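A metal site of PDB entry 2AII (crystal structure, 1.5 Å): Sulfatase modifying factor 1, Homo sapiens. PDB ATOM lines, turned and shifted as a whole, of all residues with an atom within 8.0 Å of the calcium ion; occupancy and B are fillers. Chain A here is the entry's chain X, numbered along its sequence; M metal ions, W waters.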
ATOM      1  N   TYR A  44      17.339   8.170 -18.639  1.00  0.00           N
ATOM      2  CA  TYR A  44      17.020   9.477 -19.206  1.00  0.00           C
ATOM      3  C   TYR A  44      16.600   9.337 -20.664  1.00  0.00           C
ATOM      4  O   TYR A  44      17.073   8.457 -21.400  1.00  0.00           O
ATOM      5  CB  TYR A  44      18.266  10.379 -19.191  1.00  0.00           C
ATOM      6  CG  TYR A  44      18.965  10.421 -17.860  1.00  0.00           C
ATOM      7  CD1 TYR A  44      18.400  11.080 -16.784  1.00  0.00           C
ATOM      8  CD2 TYR A  44      20.195   9.774 -17.663  1.00  0.00           C
ATOM      9  CE1 TYR A  44      19.014  11.110 -15.560  1.00  0.00           C
ATOM     10  CE2 TYR A  44      20.805   9.807 -16.431  1.00  0.00           C
ATOM     11  CZ  TYR A  44      20.230  10.482 -15.392  1.00  0.00           C
ATOM     12  OH  TYR A  44      20.830  10.522 -14.143  1.00  0.00           O
ATOM     13  N   GLU A  45      15.764  10.269 -21.106  1.00  0.00           N
ATOM     14  CA  GLU A  45      15.594  10.489 -22.542  1.00  0.00           C
ATOM     15  C   GLU A  45      16.966  10.736 -23.141  1.00  0.00           C
ATOM     16  O   GLU A  45      17.849  11.305 -22.496  1.00  0.00           O
ATOM     17  CB  GLU A  45      14.734  11.723 -22.772  1.00  0.00           C
ATOM     18  CG  GLU A  45      13.299  11.606 -22.241  1.00  0.00           C
ATOM     19  CD  GLU A  45      12.662  12.949 -21.882  1.00  0.00           C
ATOM     20  OE1 GLU A  45      13.381  13.831 -21.397  1.00  0.00           O
ATOM     21  OE2 GLU A  45      11.420  13.093 -22.062  1.00  0.00           O
ATOM     22  N   PRO A 120      16.362  16.776 -23.978  1.00  0.00           N
ATOM     23  CA  PRO A 120      16.128  15.657 -24.883  1.00  0.00           C
ATOM     24  C   PRO A 120      16.287  16.059 -26.331  1.00  0.00           C
ATOM     25  O   PRO A 120      15.844  17.147 -26.713  1.00  0.00           O
ATOM     26  CB  PRO A 120      14.670  15.273 -24.582  1.00  0.00           C
ATOM     27  CG  PRO A 120      14.049  16.506 -23.991  1.00  0.00           C
ATOM     28  CD  PRO A 120      15.168  17.103 -23.183  1.00  0.00           C
ATOM     29  N   TRP A 146       7.870  -0.308 -21.901  1.00  0.00           N
ATOM     30  CA  TRP A 146       7.841   1.111 -21.630  1.00  0.00           C
ATOM     31  C   TRP A 146       6.830   1.395 -20.511  1.00  0.00           C
ATOM     32  O   TRP A 146       7.127   2.097 -19.534  1.00  0.00           O
ATOM     33  CB  TRP A 146       7.541   1.907 -22.914  1.00  0.00           C
ATOM     34  CG  TRP A 146       7.715   3.370 -22.694  1.00  0.00           C
ATOM     35  CD1 TRP A 146       8.795   4.128 -23.046  1.00  0.00           C
ATOM     36  CD2 TRP A 146       6.789   4.258 -22.040  1.00  0.00           C
ATOM     37  NE1 TRP A 146       8.590   5.433 -22.641  1.00  0.00           N
ATOM     38  CE2 TRP A 146       7.374   5.536 -22.031  1.00  0.00           C
ATOM     39  CE3 TRP A 146       5.525   4.082 -21.471  1.00  0.00           C
ATOM     40  CZ2 TRP A 146       6.763   6.623 -21.444  1.00  0.00           C
ATOM     41  CZ3 TRP A 146       4.914   5.161 -20.880  1.00  0.00           C
ATOM     42  CH2 TRP A 146       5.527   6.418 -20.870  1.00  0.00           C
ATOM     43  N   ASN A 174       7.338  17.617 -16.407  1.00  0.00           N
ATOM     44  CA  ASN A 174       7.241  18.810 -17.241  1.00  0.00           C
ATOM     45  C   ASN A 174       6.118  18.680 -18.258  1.00  0.00           C
ATOM     46  O   ASN A 174       6.256  18.031 -19.277  1.00  0.00           O
ATOM     47  CB  ASN A 174       8.568  19.050 -17.963  1.00  0.00           C
ATOM     48  CG  ASN A 174       8.542  20.252 -18.858  1.00  0.00           C
ATOM     49  OD1 ASN A 174       7.714  21.134 -18.690  1.00  0.00           O
ATOM     50  ND2 ASN A 174       9.468  20.311 -19.831  1.00  0.00           N
ATOM     51  N   TYR A 207      13.699   9.058 -15.191  1.00  0.00           N
ATOM     52  CA  TYR A 207      13.417  10.502 -15.203  1.00  0.00           C
ATOM     53  C   TYR A 207      12.586  10.835 -16.429  1.00  0.00           C
ATOM     54  O   TYR A 207      12.881  10.334 -17.509  1.00  0.00           O
ATOM     55  CB  TYR A 207      14.747  11.272 -15.241  1.00  0.00           C
ATOM     56  CG  TYR A 207      15.570  11.137 -13.996  1.00  0.00           C
ATOM     57  CD1 TYR A 207      16.329  10.001 -13.756  1.00  0.00           C
ATOM     58  CD2 TYR A 207      15.504  12.115 -13.018  1.00  0.00           C
ATOM     59  CE1 TYR A 207      17.053   9.864 -12.592  1.00  0.00           C
ATOM     60  CE2 TYR A 207      16.231  11.993 -11.847  1.00  0.00           C
ATOM     61  CZ  TYR A 207      17.017  10.873 -11.648  1.00  0.00           C
ATOM     62  OH  TYR A 207      17.759  10.723 -10.468  1.00  0.00           O
ATOM     63  N   ASN A 208      11.589  11.709 -16.257  1.00  0.00           N
ATOM     64  CA  ASN A 208      10.809  12.296 -17.355  1.00  0.00           C
ATOM     65  C   ASN A 208      10.210  11.273 -18.266  1.00  0.00           C
ATOM     66  O   ASN A 208      10.017  11.517 -19.441  1.00  0.00           O
ATOM     67  CB  ASN A 208      11.665  13.306 -18.098  1.00  0.00           C
ATOM     68  CG  ASN A 208      12.114  14.428 -17.194  1.00  0.00           C
ATOM     69  OD1 ASN A 208      11.291  15.186 -16.684  1.00  0.00           O
ATOM     70  ND2 ASN A 208      13.440  14.513 -16.943  1.00  0.00           N
ATOM     71  N   ILE A 209       9.796  10.142 -17.671  1.00  0.00           N
ATOM     72  CA  ILE A 209       9.134   9.124 -18.447  1.00  0.00           C
ATOM     73  C   ILE A 209       7.704   9.545 -18.809  1.00  0.00           C
ATOM     74  O   ILE A 209       7.217   9.201 -19.894  1.00  0.00           O
ATOM     75  CB  ILE A 209       9.263   7.721 -17.799  1.00  0.00           C
ATOM     76  CG1 ILE A 209       8.788   6.651 -18.778  1.00  0.00           C
ATOM     77  CG2 ILE A 209       8.558   7.644 -16.478  1.00  0.00           C
ATOM     78  CD1 ILE A 209       9.497   5.322 -18.656  1.00  0.00           C
ATOM     79  N   VAL A 210       7.036  10.332 -17.961  1.00  0.00           N
ATOM     80  CA  VAL A 210       5.903  11.136 -18.445  1.00  0.00           C
ATOM     81  C   VAL A 210       6.345  12.598 -18.588  1.00  0.00           C
ATOM     82  O   VAL A 210       7.171  13.091 -17.793  1.00  0.00           O
ATOM     83  CB  VAL A 210       4.606  11.043 -17.609  1.00  0.00           C
ATOM     84  CG1 VAL A 210       4.074   9.642 -17.582  1.00  0.00           C
ATOM     85  CG2 VAL A 210       4.783  11.537 -16.238  1.00  0.00           C
ATOM     86  N   GLY A 211       5.834  13.265 -19.602  1.00  0.00           N
ATOM     87  CA  GLY A 211       6.243  14.617 -19.877  1.00  0.00           C
ATOM     88  C   GLY A 211       7.593  14.790 -20.531  1.00  0.00           C
ATOM     89  O   GLY A 211       8.318  13.829 -20.872  1.00  0.00           O
ATOM     90  N   ASN A 212       7.909  16.063 -20.726  1.00  0.00           N
ATOM     91  CA  ASN A 212       9.147  16.517 -21.360  1.00  0.00           C
ATOM     92  C   ASN A 212       9.069  16.218 -22.846  1.00  0.00           C
ATOM     93  O   ASN A 212       8.357  16.942 -23.532  1.00  0.00           O
ATOM     94  CB  ASN A 212      10.400  16.017 -20.631  1.00  0.00           C
ATOM     95  CG  ASN A 212      11.534  17.039 -20.672  1.00  0.00           C
ATOM     96  OD1 ASN A 212      11.286  18.242 -20.681  1.00  0.00           O
ATOM     97  ND2 ASN A 212      12.775  16.562 -20.631  1.00  0.00           N
ATOM     98  N   ALA A 213       9.710  15.164 -23.344  1.00  0.00           N
ATOM     99  CA  ALA A 213       9.486  14.703 -24.732  1.00  0.00           C
ATOM    100  C   ALA A 213       8.637  13.415 -24.704  1.00  0.00           C
ATOM    101  O   ALA A 213       8.806  12.572 -23.823  1.00  0.00           O
ATOM    102  CB  ALA A 213      10.821  14.408 -25.435  1.00  0.00           C
ATOM    103  N   TRP A 214       7.734  13.286 -25.681  1.00  0.00           N
ATOM    104  CA  TRP A 214       7.135  12.009 -26.033  1.00  0.00           C
ATOM    105  C   TRP A 214       8.240  10.994 -26.328  1.00  0.00           C
ATOM    106  O   TRP A 214       9.352  11.380 -26.718  1.00  0.00           O
ATOM    107  CB  TRP A 214       6.291  12.124 -27.318  1.00  0.00           C
ATOM    108  CG  TRP A 214       4.929  12.674 -27.190  1.00  0.00           C
ATOM    109  CD1 TRP A 214       4.506  13.942 -27.454  1.00  0.00           C
ATOM    110  CD2 TRP A 214       3.733  11.920 -26.883  1.00  0.00           C
ATOM    111  NE1 TRP A 214       3.137  14.046 -27.305  1.00  0.00           N
ATOM    112  CE2 TRP A 214       2.644  12.818 -26.949  1.00  0.00           C
ATOM    113  CE3 TRP A 214       3.493  10.588 -26.568  1.00  0.00           C
ATOM    114  CZ2 TRP A 214       1.322  12.414 -26.684  1.00  0.00           C
ATOM    115  CZ3 TRP A 214       2.171  10.175 -26.299  1.00  0.00           C
ATOM    116  CH2 TRP A 214       1.116  11.101 -26.357  1.00  0.00           C
ATOM    117  N   GLU A 215       7.916   9.699 -26.202  1.00  0.00           N
ATOM    118  CA  GLU A 215       8.914   8.677 -26.407  1.00  0.00           C
ATOM    119  C   GLU A 215       8.450   7.583 -27.344  1.00  0.00           C
ATOM    120  O   GLU A 215       7.439   6.939 -27.089  1.00  0.00           O
ATOM    121  CB  GLU A 215       9.316   8.115 -25.043  1.00  0.00           C
ATOM    122  CG  GLU A 215       9.805   9.242 -24.156  1.00  0.00           C
ATOM    123  CD  GLU A 215      10.224   8.844 -22.732  1.00  0.00           C
ATOM    124  OE1 GLU A 215      10.418   7.651 -22.486  1.00  0.00           O
ATOM    125  OE2 GLU A 215      10.398   9.785 -21.908  1.00  0.00           O
ATOM    126  N   LYS A 245       4.672   7.057 -26.373  1.00  0.00           N
ATOM    127  CA  LYS A 245       4.133   7.045 -25.008  1.00  0.00           C
ATOM    128  C   LYS A 245       4.622   8.240 -24.188  1.00  0.00           C
ATOM    129  O   LYS A 245       5.652   8.869 -24.500  1.00  0.00           O
ATOM    130  CB  LYS A 245       4.567   5.774 -24.291  1.00  0.00           C
ATOM    131  CG  LYS A 245       4.036   4.476 -24.904  1.00  0.00           C
ATOM    132  CD  LYS A 245       2.580   4.196 -24.549  1.00  0.00           C
ATOM    133  CE  LYS A 245       2.414   3.553 -23.183  1.00  0.00           C
ATOM    134  NZ  LYS A 245       1.007   2.998 -22.988  1.00  0.00           N
ATOM    135  N   GLY A 246       3.848   8.535 -23.146  1.00  0.00           N
ATOM    136  CA  GLY A 246       4.325   9.373 -22.051  1.00  0.00           C
ATOM    137  C   GLY A 246       3.956  10.836 -22.034  1.00  0.00           C
ATOM    138  O   GLY A 246       4.082  11.487 -20.998  1.00  0.00           O
ATOM    139  N   GLY A 247       3.508  11.359 -23.171  1.00  0.00           N
ATOM    140  CA  GLY A 247       3.253  12.798 -23.289  1.00  0.00           C
ATOM    141  C   GLY A 247       4.505  13.670 -23.195  1.00  0.00           C
ATOM    142  O   GLY A 247       5.630  13.191 -23.121  1.00  0.00           O
ATOM    143  N   SER A 248       4.277  14.971 -23.235  1.00  0.00           N
ATOM    144  CA  SER A 248       5.311  15.967 -23.386  1.00  0.00           C
ATOM    145  C   SER A 248       5.019  17.240 -22.596  1.00  0.00           C
ATOM    146  O   SER A 248       3.996  17.356 -21.892  1.00  0.00           O
ATOM    147  CB  SER A 248       5.450  16.330 -24.866  1.00  0.00           C
ATOM    148  OG  SER A 248       4.394  17.186 -25.277  1.00  0.00           O
ATOM    149  N   TYR A 249       5.902  18.195 -22.765  1.00  0.00           N
ATOM    150  CA  TYR A 249       5.778  19.509 -22.144  1.00  0.00           C
ATOM    151  C   TYR A 249       4.536  20.271 -22.586  1.00  0.00           C
ATOM    152  O   TYR A 249       4.171  21.287 -21.973  1.00  0.00           O
ATOM    153  CB  TYR A 249       7.027  20.348 -22.421  1.00  0.00           C
ATOM    154  CG  TYR A 249       7.275  20.765 -23.850  1.00  0.00           C
ATOM    155  CD1 TYR A 249       8.226  20.108 -24.628  1.00  0.00           C
ATOM    156  CD2 TYR A 249       6.603  21.847 -24.398  1.00  0.00           C
ATOM    157  CE1 TYR A 249       8.466  20.517 -25.934  1.00  0.00           C
ATOM    158  CE2 TYR A 249       6.852  22.259 -25.701  1.00  0.00           C
ATOM    159  CZ  TYR A 249       7.781  21.592 -26.450  1.00  0.00           C
ATOM    160  OH  TYR A 249       8.048  21.990 -27.760  1.00  0.00           O
ATOM    161  N   ASN A 275       8.312  17.994 -29.973  1.00  0.00           N
ATOM    162  CA  ASN A 275       7.996  17.448 -28.663  1.00  0.00           C
ATOM    163  C   ASN A 275       8.148  15.934 -28.572  1.00  0.00           C
ATOM    164  O   ASN A 275       7.616  15.323 -27.644  1.00  0.00           O
ATOM    165  CB  ASN A 275       6.573  17.842 -28.228  1.00  0.00           C
ATOM    166  CG  ASN A 275       5.502  17.125 -28.992  1.00  0.00           C
ATOM    167  OD1 ASN A 275       5.761  16.545 -30.046  1.00  0.00           O
ATOM    168  ND2 ASN A 275       4.254  17.170 -28.475  1.00  0.00           N
ATOM    169  N   GLY A 277      10.823  12.620 -28.730  1.00  0.00           N
ATOM    170  CA  GLY A 277      12.161  12.033 -28.608  1.00  0.00           C
ATOM    171  C   GLY A 277      12.024  10.558 -28.281  1.00  0.00           C
ATOM    172  O   GLY A 277      11.104   9.872 -28.772  1.00  0.00           O
ATOM    173  N   PHE A 278      12.936  10.060 -27.455  1.00  0.00           N
ATOM    174  CA  PHE A 278      12.989   8.631 -27.150  1.00  0.00           C
ATOM    175  C   PHE A 278      14.016   8.310 -26.087  1.00  0.00           C
ATOM    176  O   PHE A 278      14.881   9.153 -25.772  1.00  0.00           O
ATOM    177  CB  PHE A 278      13.288   7.793 -28.401  1.00  0.00           C
ATOM    178  CG  PHE A 278      14.680   8.000 -28.946  1.00  0.00           C
ATOM    179  CD1 PHE A 278      15.666   7.041 -28.740  1.00  0.00           C
ATOM    180  CD2 PHE A 278      15.001   9.115 -29.675  1.00  0.00           C
ATOM    181  CE1 PHE A 278      16.951   7.247 -29.248  1.00  0.00           C
ATOM    182  CE2 PHE A 278      16.287   9.303 -30.175  1.00  0.00           C
ATOM    183  CZ  PHE A 278      17.248   8.380 -29.962  1.00  0.00           C
ATOM    184  N   ARG A 279      13.889   7.104 -25.527  1.00  0.00           N
ATOM    185  CA  ARG A 279      14.961   6.500 -24.734  1.00  0.00           C
ATOM    186  C   ARG A 279      15.130   5.053 -25.221  1.00  0.00           C
ATOM    187  O   ARG A 279      14.241   4.497 -25.863  1.00  0.00           O
ATOM    188  CB  ARG A 279      14.649   6.512 -23.236  1.00  0.00           C
ATOM    189  CG  ARG A 279      13.574   5.555 -22.768  1.00  0.00           C
ATOM    190  CD  ARG A 279      13.304   5.685 -21.285  1.00  0.00           C
ATOM    191  NE  ARG A 279      12.666   6.965 -21.010  1.00  0.00           N
ATOM    192  CZ  ARG A 279      12.939   7.763 -19.991  1.00  0.00           C
ATOM    193  NH1 ARG A 279      13.840   7.441 -19.075  1.00  0.00           N
ATOM    194  NH2 ARG A 279      12.291   8.916 -19.888  1.00  0.00           N
HETATM  195 CA    CA M   1       9.452  11.927 -21.674  1.00  0.00          CA
HETATM  196  O   HOH W   1       7.260  11.044 -21.914  1.00  0.00           O
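The side-chain carboxylate of Glu 45 is in hydrogen-bond range of the side-chain amide nitrogen of Asn 212 (2.9 Å). The guanidinium group (NH2) of Arg 279 sits close to the backbone carbonyl oxygen (O) of Asn 208 (3.5 Å). OE1 of Glu 215 lies within salt-bridge range of NE of Arg 279, at 2.8 Å. The backbone NH (N) of Lys 245 is in hydrogen-bond range of the backbone carbonyl oxygen (O) of Glu 215, at 2.9 Å. The side-chain carboxylate of Glu 215 lies within hydrogen-bond range of the indole nitrogen of Trp 146 (2.9 Å). The backbone NH (N) of Gly 211 lies within hydrogen-bond range of the backbone carbonyl oxygen (O) of Gly 246, at 2.9 Å.
Ile 209 touches the calcium ion. The nearest printed residue that does not touch the calcium ion is Gly 247 (4.3 Å).
The calcium ion is bound by the side-chain carboxylate (OE2) of Glu 45 (2.3 Å). O of Ala 213 is bound to the calcium ion, at 2.3 Å. The backbone carbonyl oxygen (O) of Asn 208 is bound to the calcium ion (2.3 Å). The calcium ion is bound by the side-chain carboxylate (OE2) of Glu 215, at 2.4 Å. O of Gly 211 binds the calcium ion, at 2.4 Å. Water W1 binds the calcium ion.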
